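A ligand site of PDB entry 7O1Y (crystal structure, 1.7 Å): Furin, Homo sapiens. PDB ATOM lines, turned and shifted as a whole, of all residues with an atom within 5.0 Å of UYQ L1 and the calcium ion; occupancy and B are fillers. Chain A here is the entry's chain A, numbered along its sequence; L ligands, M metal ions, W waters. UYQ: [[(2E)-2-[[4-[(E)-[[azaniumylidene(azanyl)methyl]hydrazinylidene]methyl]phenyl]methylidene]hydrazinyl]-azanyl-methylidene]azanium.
A nitrogen (N7) of UYQ L1 sits close to the side-chain carboxylate (OD1) of Asp 151, 3.4 Å away. The side-chain carboxylate of Asp 47 lies within salt-bridge range of a nitrogen (N) of UYQ L1, at 2.7 Å. N7 of UYQ L1 is in hydrogen-bond range of O of Pro 149, at 2.9 Å. OD2 of Asp 199 is in salt-bridge range of N7 of UYQ L1. A nitrogen (N6) of UYQ L1 lies within hydrogen-bond range of the backbone carbonyl oxygen (O) of Ser 146 (2.9 Å). O of Asp 84 sits at hydrogen-bond distance from N of UYQ L1 (2.9 Å). The side-chain carboxylate of Asp 46 is in salt-bridge range of a nitrogen (N1) of UYQ L1, 3.0 Å away. The backbone carbonyl oxygen of Gly 148 sits close to a nitrogen (N5) of UYQ L1, 3.1 Å away. The backbone carbonyl oxygen of Leu 120 is in hydrogen-bond range of a nitrogen (N7) of UYQ L2 (3.1 Å).
The backbone NH of Asp 194 lies within hydrogen-bond range of the backbone carbonyl oxygen of Gly 189 (3.1 Å). The side-chain carboxylate of Glu 224 sits close to the backbone NH of Gly 189, 2.8 Å away. N of His 87 lies within hydrogen-bond range of OD2 of Asp 47 (2.9 Å). O of Asp 46 is in hydrogen-bond range of N of Leu 120 (3.0 Å). ND1 of His 87 is in hydrogen-bond range of OD2 of Asp 46 (2.9 Å).
His 87 touches UYQ L1. CD1 of Leu 120 touches N1 of UYQ L1, 3.6 Å away. C of Trp 147 touches N6 of UYQ L1 (3.3 Å).
Within 4 Å of the calcium ion: Asp 151, Asp 194 and Glu 224. The nearest printed residue that does not touch the calcium ion is Asp 199 (4.4 Å).
The calcium ion is bound by water W5 (2.3 Å), the side-chain carboxylate (OD1) of Asp 151 (2.4 Å), the side-chain carboxylate (OD2) of Asp 194 (2.4 Å), the side-chain carboxylate (OE1) of Glu 224 (2.4 Å), the side-chain carboxylate (OE2) of Glu 224 (2.4 Å), water W1 (2.5 Å) and water W6 (2.5 Å). The calcium ion has seven donor atoms within binding distance.
Water W5 lies within hydrogen-bond range of the backbone carbonyl oxygen (O) of Ser 186 and the side-chain carboxylate (OD2) of Asp 199. Water W1 lies within hydrogen-bond range of O of Pro 149, O of Glu 150 and N7 of UYQ L1. Water W3 lies within hydrogen-bond range of OD2 of Asp 199 (2.7 Å), O of Ala 185 (2.8 Å) and N6 of UYQ L1 (2.9 Å). Water W4 lies within hydrogen-bond range of the side-chain carboxylate of Asp 46, a nitrogen (N1) of UYQ L1 and a ring nitrogen (ND1) of His 87.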
ATOM      1  N   ASP A  46      22.820  21.225   4.709  1.00  0.00           N
ATOM      2  CA  ASP A  46      23.105  20.027   5.499  1.00  0.00           C
ATOM      3  C   ASP A  46      22.081  19.885   6.634  1.00  0.00           C
ATOM      4  O   ASP A  46      20.877  20.004   6.375  1.00  0.00           O
ATOM      5  CB  ASP A  46      24.562  20.119   5.970  1.00  0.00           C
ATOM      6  CG  ASP A  46      25.143  18.757   6.356  1.00  0.00           C
ATOM      7  OD1 ASP A  46      24.888  18.316   7.495  1.00  0.00           O
ATOM      8  OD2 ASP A  46      25.814  18.114   5.542  1.00  0.00           O
ATOM      9  N   ASP A  47      22.519  19.640   7.869  1.00  0.00           N
ATOM     10  CA  ASP A  47      21.603  19.328   8.981  1.00  0.00           C
ATOM     11  C   ASP A  47      21.336  20.531   9.876  1.00  0.00           C
ATOM     12  O   ASP A  47      20.784  20.354  10.972  1.00  0.00           O
ATOM     13  CB  ASP A  47      22.137  18.181   9.835  1.00  0.00           C
ATOM     14  CG  ASP A  47      23.540  18.434  10.361  1.00  0.00           C
ATOM     15  OD1 ASP A  47      23.967  19.607  10.385  1.00  0.00           O
ATOM     16  OD2 ASP A  47      24.243  17.439  10.692  1.00  0.00           O
ATOM     17  N   ASP A  84      23.856  13.769  16.353  1.00  0.00           N
ATOM     18  CA  ASP A  84      23.685  13.454  14.929  1.00  0.00           C
ATOM     19  C   ASP A  84      23.702  14.689  14.032  1.00  0.00           C
ATOM     20  O   ASP A  84      24.114  14.604  12.871  1.00  0.00           O
ATOM     21  CB  ASP A  84      22.342  12.753  14.707  1.00  0.00           C
ATOM     22  CG  ASP A  84      22.139  11.594  15.619  1.00  0.00           C
ATOM     23  OD1 ASP A  84      21.765  11.819  16.782  1.00  0.00           O
ATOM     24  OD2 ASP A  84      22.382  10.454  15.172  1.00  0.00           O
ATOM     25  N   ASN A  85      23.222  15.829  14.525  1.00  0.00           N
ATOM     26  CA  ASN A  85      23.060  17.019  13.696  1.00  0.00           C
ATOM     27  C   ASN A  85      24.174  18.030  13.885  1.00  0.00           C
ATOM     28  O   ASN A  85      23.945  19.233  13.864  1.00  0.00           O
ATOM     29  CB  ASN A  85      21.698  17.623  13.966  1.00  0.00           C
ATOM     30  CG  ASN A  85      20.591  16.711  13.541  1.00  0.00           C
ATOM     31  OD1 ASN A  85      20.495  16.315  12.370  1.00  0.00           O
ATOM     32  ND2 ASN A  85      19.761  16.305  14.501  1.00  0.00           N
ATOM     33  N   HIS A  87      26.887  18.076  11.805  1.00  0.00           N
ATOM     34  CA  HIS A  87      27.746  18.092  10.626  1.00  0.00           C
ATOM     35  C   HIS A  87      27.735  19.454   9.923  1.00  0.00           C
ATOM     36  O   HIS A  87      28.778  19.926   9.466  1.00  0.00           O
ATOM     37  CB  HIS A  87      27.322  16.983   9.669  1.00  0.00           C
ATOM     38  CG  HIS A  87      28.253  16.790   8.525  1.00  0.00           C
ATOM     39  ND1 HIS A  87      27.953  17.203   7.236  1.00  0.00           N
ATOM     40  CD2 HIS A  87      29.493  16.243   8.474  1.00  0.00           C
ATOM     41  CE1 HIS A  87      28.971  16.902   6.445  1.00  0.00           C
ATOM     42  NE2 HIS A  87      29.917  16.330   7.176  1.00  0.00           N
ATOM     43  N   LEU A 120      18.599  18.179   5.869  1.00  0.00           N
ATOM     44  CA  LEU A 120      18.815  16.737   5.906  1.00  0.00           C
ATOM     45  C   LEU A 120      18.122  16.052   7.084  1.00  0.00           C
ATOM     46  O   LEU A 120      18.127  14.807   7.159  1.00  0.00           O
ATOM     47  CB  LEU A 120      20.297  16.399   5.998  1.00  0.00           C
ATOM     48  CG  LEU A 120      21.109  16.677   4.730  1.00  0.00           C
ATOM     49  CD1 LEU A 120      22.567  16.279   4.927  1.00  0.00           C
ATOM     50  CD2 LEU A 120      20.514  15.995   3.497  1.00  0.00           C
ATOM     51  N   SER A 146      27.089  17.808   0.396  1.00  0.00           N
ATOM     52  CA  SER A 146      27.760  16.532   0.241  1.00  0.00           C
ATOM     53  C   SER A 146      26.796  15.348   0.266  1.00  0.00           C
ATOM     54  O   SER A 146      27.222  14.212   0.529  1.00  0.00           O
ATOM     55  CB  SER A 146      28.850  16.301   1.328  1.00  0.00           C
ATOM     56  OG  SER A 146      28.326  16.553   2.624  1.00  0.00           O
ATOM     57  N   TRP A 147      25.536  15.574  -0.068  1.00  0.00           N
ATOM     58  CA  TRP A 147      24.504  14.541  -0.127  1.00  0.00           C
ATOM     59  C   TRP A 147      24.122  14.189  -1.560  1.00  0.00           C
ATOM     60  O   TRP A 147      24.519  14.832  -2.542  1.00  0.00           O
ATOM     61  CB  TRP A 147      23.266  14.997   0.663  1.00  0.00           C
ATOM     62  CG  TRP A 147      22.897  16.458   0.456  1.00  0.00           C
ATOM     63  CD1 TRP A 147      23.320  17.518   1.231  1.00  0.00           C
ATOM     64  CD2 TRP A 147      22.073  17.036  -0.576  1.00  0.00           C
ATOM     65  NE1 TRP A 147      22.800  18.690   0.759  1.00  0.00           N
ATOM     66  CE2 TRP A 147      22.047  18.432  -0.368  1.00  0.00           C
ATOM     67  CE3 TRP A 147      21.358  16.500  -1.663  1.00  0.00           C
ATOM     68  CZ2 TRP A 147      21.316  19.294  -1.177  1.00  0.00           C
ATOM     69  CZ3 TRP A 147      20.649  17.368  -2.466  1.00  0.00           C
ATOM     70  CH2 TRP A 147      20.621  18.745  -2.216  1.00  0.00           C
ATOM     71  N   GLY A 148      23.318  13.148  -1.673  1.00  0.00           N
ATOM     72  CA  GLY A 148      23.036  12.505  -2.933  1.00  0.00           C
ATOM     73  C   GLY A 148      22.675  11.066  -2.689  1.00  0.00           C
ATOM     74  O   GLY A 148      22.444  10.645  -1.544  1.00  0.00           O
ATOM     75  N   PRO A 149      22.655  10.257  -3.751  1.00  0.00           N
ATOM     76  CA  PRO A 149      22.205   8.871  -3.596  1.00  0.00           C
ATOM     77  C   PRO A 149      23.131   8.100  -2.666  1.00  0.00           C
ATOM     78  O   PRO A 149      24.300   8.427  -2.502  1.00  0.00           O
ATOM     79  CB  PRO A 149      22.240   8.310  -5.026  1.00  0.00           C
ATOM     80  CG  PRO A 149      23.159   9.227  -5.787  1.00  0.00           C
ATOM     81  CD  PRO A 149      23.001  10.580  -5.143  1.00  0.00           C
ATOM     82  N   GLU A 150      22.574   7.051  -2.067  1.00  0.00           N
ATOM     83  CA  GLU A 150      23.357   6.246  -1.125  1.00  0.00           C
ATOM     84  C   GLU A 150      24.668   5.798  -1.755  1.00  0.00           C
ATOM     85  O   GLU A 150      24.714   5.379  -2.926  1.00  0.00           O
ATOM     86  CB  GLU A 150      22.556   5.015  -0.689  1.00  0.00           C
ATOM     87  CG  GLU A 150      21.324   5.346   0.194  1.00  0.00           C
ATOM     88  CD  GLU A 150      21.656   6.010   1.537  1.00  0.00           C
ATOM     89  OE1 GLU A 150      20.729   6.598   2.148  1.00  0.00           O
ATOM     90  OE2 GLU A 150      22.824   5.956   2.013  1.00  0.00           O
ATOM     91  N   ASP A 151      25.735   5.886  -0.964  1.00  0.00           N
ATOM     92  CA  ASP A 151      27.079   5.471  -1.387  1.00  0.00           C
ATOM     93  C   ASP A 151      27.260   3.972  -1.130  1.00  0.00           C
ATOM     94  O   ASP A 151      28.227   3.538  -0.506  1.00  0.00           O
ATOM     95  CB  ASP A 151      28.140   6.281  -0.650  1.00  0.00           C
ATOM     96  CG  ASP A 151      28.247   7.699  -1.149  1.00  0.00           C
ATOM     97  OD1 ASP A 151      27.942   7.895  -2.341  1.00  0.00           O
ATOM     98  OD2 ASP A 151      28.687   8.588  -0.383  1.00  0.00           O
ATOM     99  N   ALA A 185      30.747  17.540  -2.819  1.00  0.00           N
ATOM    100  CA  ALA A 185      31.637  16.420  -2.523  1.00  0.00           C
ATOM    101  C   ALA A 185      31.349  15.254  -3.458  1.00  0.00           C
ATOM    102  O   ALA A 185      30.201  14.916  -3.727  1.00  0.00           O
ATOM    103  CB  ALA A 185      31.438  16.005  -1.070  1.00  0.00           C
ATOM    104  N   SER A 186      32.413  14.570  -3.925  1.00  0.00           N
ATOM    105  CA  SER A 186      32.215  13.518  -4.926  1.00  0.00           C
ATOM    106  C   SER A 186      31.712  12.197  -4.330  1.00  0.00           C
ATOM    107  O   SER A 186      31.397  11.286  -5.114  1.00  0.00           O
ATOM    108  CB  SER A 186      33.500  13.288  -5.688  1.00  0.00           C
ATOM    109  OG  SER A 186      34.566  12.925  -4.807  1.00  0.00           O
ATOM    110  N   GLY A 187      31.618  12.063  -3.009  1.00  0.00           N
ATOM    111  CA  GLY A 187      31.053  10.859  -2.396  1.00  0.00           C
ATOM    112  C   GLY A 187      31.978  10.248  -1.347  1.00  0.00           C
ATOM    113  O   GLY A 187      33.163  10.543  -1.255  1.00  0.00           O
ATOM    114  N   GLY A 189      31.785   6.595  -0.871  1.00  0.00           N
ATOM    115  CA  GLY A 189      31.538   5.178  -1.130  1.00  0.00           C
ATOM    116  C   GLY A 189      32.744   4.312  -1.472  1.00  0.00           C
ATOM    117  O   GLY A 189      32.585   3.200  -1.993  1.00  0.00           O
ATOM    118  N   ASP A 194      32.388   2.200  -4.916  1.00  0.00           N
ATOM    119  CA  ASP A 194      31.463   3.046  -5.676  1.00  0.00           C
ATOM    120  C   ASP A 194      32.249   3.850  -6.708  1.00  0.00           C
ATOM    121  O   ASP A 194      33.465   4.074  -6.569  1.00  0.00           O
ATOM    122  CB  ASP A 194      30.701   3.954  -4.712  1.00  0.00           C
ATOM    123  CG  ASP A 194      29.420   4.508  -5.282  1.00  0.00           C
ATOM    124  OD1 ASP A 194      29.087   4.252  -6.471  1.00  0.00           O
ATOM    125  OD2 ASP A 194      28.716   5.222  -4.525  1.00  0.00           O
ATOM    126  N   CYS A 196      31.825   7.381  -8.951  1.00  0.00           N
ATOM    127  CA  CYS A 196      30.940   8.491  -8.620  1.00  0.00           C
ATOM    128  C   CYS A 196      30.225   9.129  -9.811  1.00  0.00           C
ATOM    129  O   CYS A 196      29.373   9.999  -9.592  1.00  0.00           O
ATOM    130  CB  CYS A 196      31.671   9.591  -7.810  1.00  0.00           C
ATOM    131  SG  CYS A 196      33.453  10.009  -8.183  1.00  0.00           S
ATOM    132  N   ASP A 199      26.485   9.092  -9.470  1.00  0.00           N
ATOM    133  CA  ASP A 199      25.858  10.089  -8.599  1.00  0.00           C
ATOM    134  C   ASP A 199      25.619  11.333  -9.438  1.00  0.00           C
ATOM    135  O   ASP A 199      26.567  12.055  -9.775  1.00  0.00           O
ATOM    136  CB  ASP A 199      26.771  10.333  -7.404  1.00  0.00           C
ATOM    137  CG  ASP A 199      26.412  11.568  -6.567  1.00  0.00           C
ATOM    138  OD1 ASP A 199      25.537  12.374  -6.919  1.00  0.00           O
ATOM    139  OD2 ASP A 199      27.083  11.736  -5.527  1.00  0.00           O
ATOM    140  N   GLU A 224      35.818   8.033  -3.862  1.00  0.00           N
ATOM    141  CA  GLU A 224      35.321   7.466  -5.112  1.00  0.00           C
ATOM    142  C   GLU A 224      36.045   8.121  -6.263  1.00  0.00           C
ATOM    143  O   GLU A 224      36.197   9.352  -6.280  1.00  0.00           O
ATOM    144  CB  GLU A 224      33.814   7.683  -5.277  1.00  0.00           C
ATOM    145  CG  GLU A 224      32.970   7.071  -4.129  1.00  0.00           C
ATOM    146  CD  GLU A 224      31.465   7.358  -4.307  1.00  0.00           C
ATOM    147  OE1 GLU A 224      30.790   7.654  -3.273  1.00  0.00           O
ATOM    148  OE2 GLU A 224      30.962   7.269  -5.454  1.00  0.00           O
HETATM  149  N1  UYQ L   1      24.369  15.438   7.903  1.00  0.00           N
HETATM  150  C7  UYQ L   1      26.151  11.088  -1.838  1.00  0.00           C
HETATM  151  C8  UYQ L   1      23.867   9.756   3.461  1.00  0.00           C
HETATM  152  N2  UYQ L   1      23.614  13.304   8.300  1.00  0.00           N
HETATM  153  C9  UYQ L   1      23.638  10.133   4.771  1.00  0.00           C
HETATM  154  C1  UYQ L   1      23.658  11.835   6.584  1.00  0.00           C
HETATM  155  C5  UYQ L   1      24.380  10.656   2.527  1.00  0.00           C
HETATM  156  C6  UYQ L   1      24.727  10.201   1.181  1.00  0.00           C
HETATM  157  N3  UYQ L   1      23.904  13.022   6.978  1.00  0.00           N
HETATM  158  C4  UYQ L   1      24.660  11.950   2.965  1.00  0.00           C
HETATM  159  C3  UYQ L   1      24.432  12.326   4.276  1.00  0.00           C
HETATM  160  C2  UYQ L   1      23.917  11.426   5.199  1.00  0.00           C
HETATM  161  N4  UYQ L   1      25.376  10.941   0.362  1.00  0.00           N
HETATM  162  N   UYQ L   1      23.609  14.862   9.998  1.00  0.00           N
HETATM  163  C   UYQ L   1      23.869  14.549   8.732  1.00  0.00           C
HETATM  164  N5  UYQ L   1      25.480  10.395  -0.896  1.00  0.00           N
HETATM  165  N6  UYQ L   1      26.777  12.202  -1.508  1.00  0.00           N
HETATM  166  N7  UYQ L   1      26.081  10.695  -3.083  1.00  0.00           N
HETATM  167  N1  UYQ L   2      18.097  11.674  -5.796  1.00  0.00           N
HETATM  168  C7  UYQ L   2      20.331  11.024   7.183  1.00  0.00           C
HETATM  169  C8  UYQ L   2      19.935  12.301   2.231  1.00  0.00           C
HETATM  170  N2  UYQ L   2      18.735  12.117  -3.634  1.00  0.00           N
HETATM  171  C9  UYQ L   2      19.687  12.796   0.963  1.00  0.00           C
HETATM  172  C1  UYQ L   2      19.323  12.450  -1.473  1.00  0.00           C
HETATM  173  C5  UYQ L   2      20.226  10.958   2.437  1.00  0.00           C
HETATM  174  C6  UYQ L   2      20.394  10.384   3.779  1.00  0.00           C
HETATM  175  N3  UYQ L   2      19.244  11.633  -2.446  1.00  0.00           N
HETATM  176  C4  UYQ L   2      20.289  10.135   1.312  1.00  0.00           C
HETATM  177  C3  UYQ L   2      20.027  10.632   0.047  1.00  0.00           C
HETATM  178  C2  UYQ L   2      19.716  11.969  -0.146  1.00  0.00           C
HETATM  179  N4  UYQ L   2      20.328  11.106   4.836  1.00  0.00           N
HETATM  180  N   UYQ L   2      18.759   9.953  -4.413  1.00  0.00           N
HETATM  181  C   UYQ L   2      18.522  11.237  -4.616  1.00  0.00           C
HETATM  182  N5  UYQ L   2      20.549  10.411   6.000  1.00  0.00           N
HETATM  183  N6  UYQ L   2      20.552  10.349   8.296  1.00  0.00           N
HETATM  184  N7  UYQ L   2      19.919  12.275   7.218  1.00  0.00           N
HETATM  185 CA    CA M   1      28.733   7.616  -4.546  1.00  0.00          CA
HETATM  186  O   HOH W   1      26.279   7.620  -4.628  1.00  0.00           O
HETATM  187  O   HOH W   2      23.286  11.510  10.578  1.00  0.00           O
HETATM  188  O   HOH W   3      27.745  13.647  -3.773  1.00  0.00           O
HETATM  189  O   HOH W   4      25.867  15.451   5.173  1.00  0.00           O
HETATM  190  O   HOH W   5      29.150   9.849  -5.137  1.00  0.00           O
HETATM  191  O   HOH W   6      28.156   6.943  -6.924  1.00  0.00           O
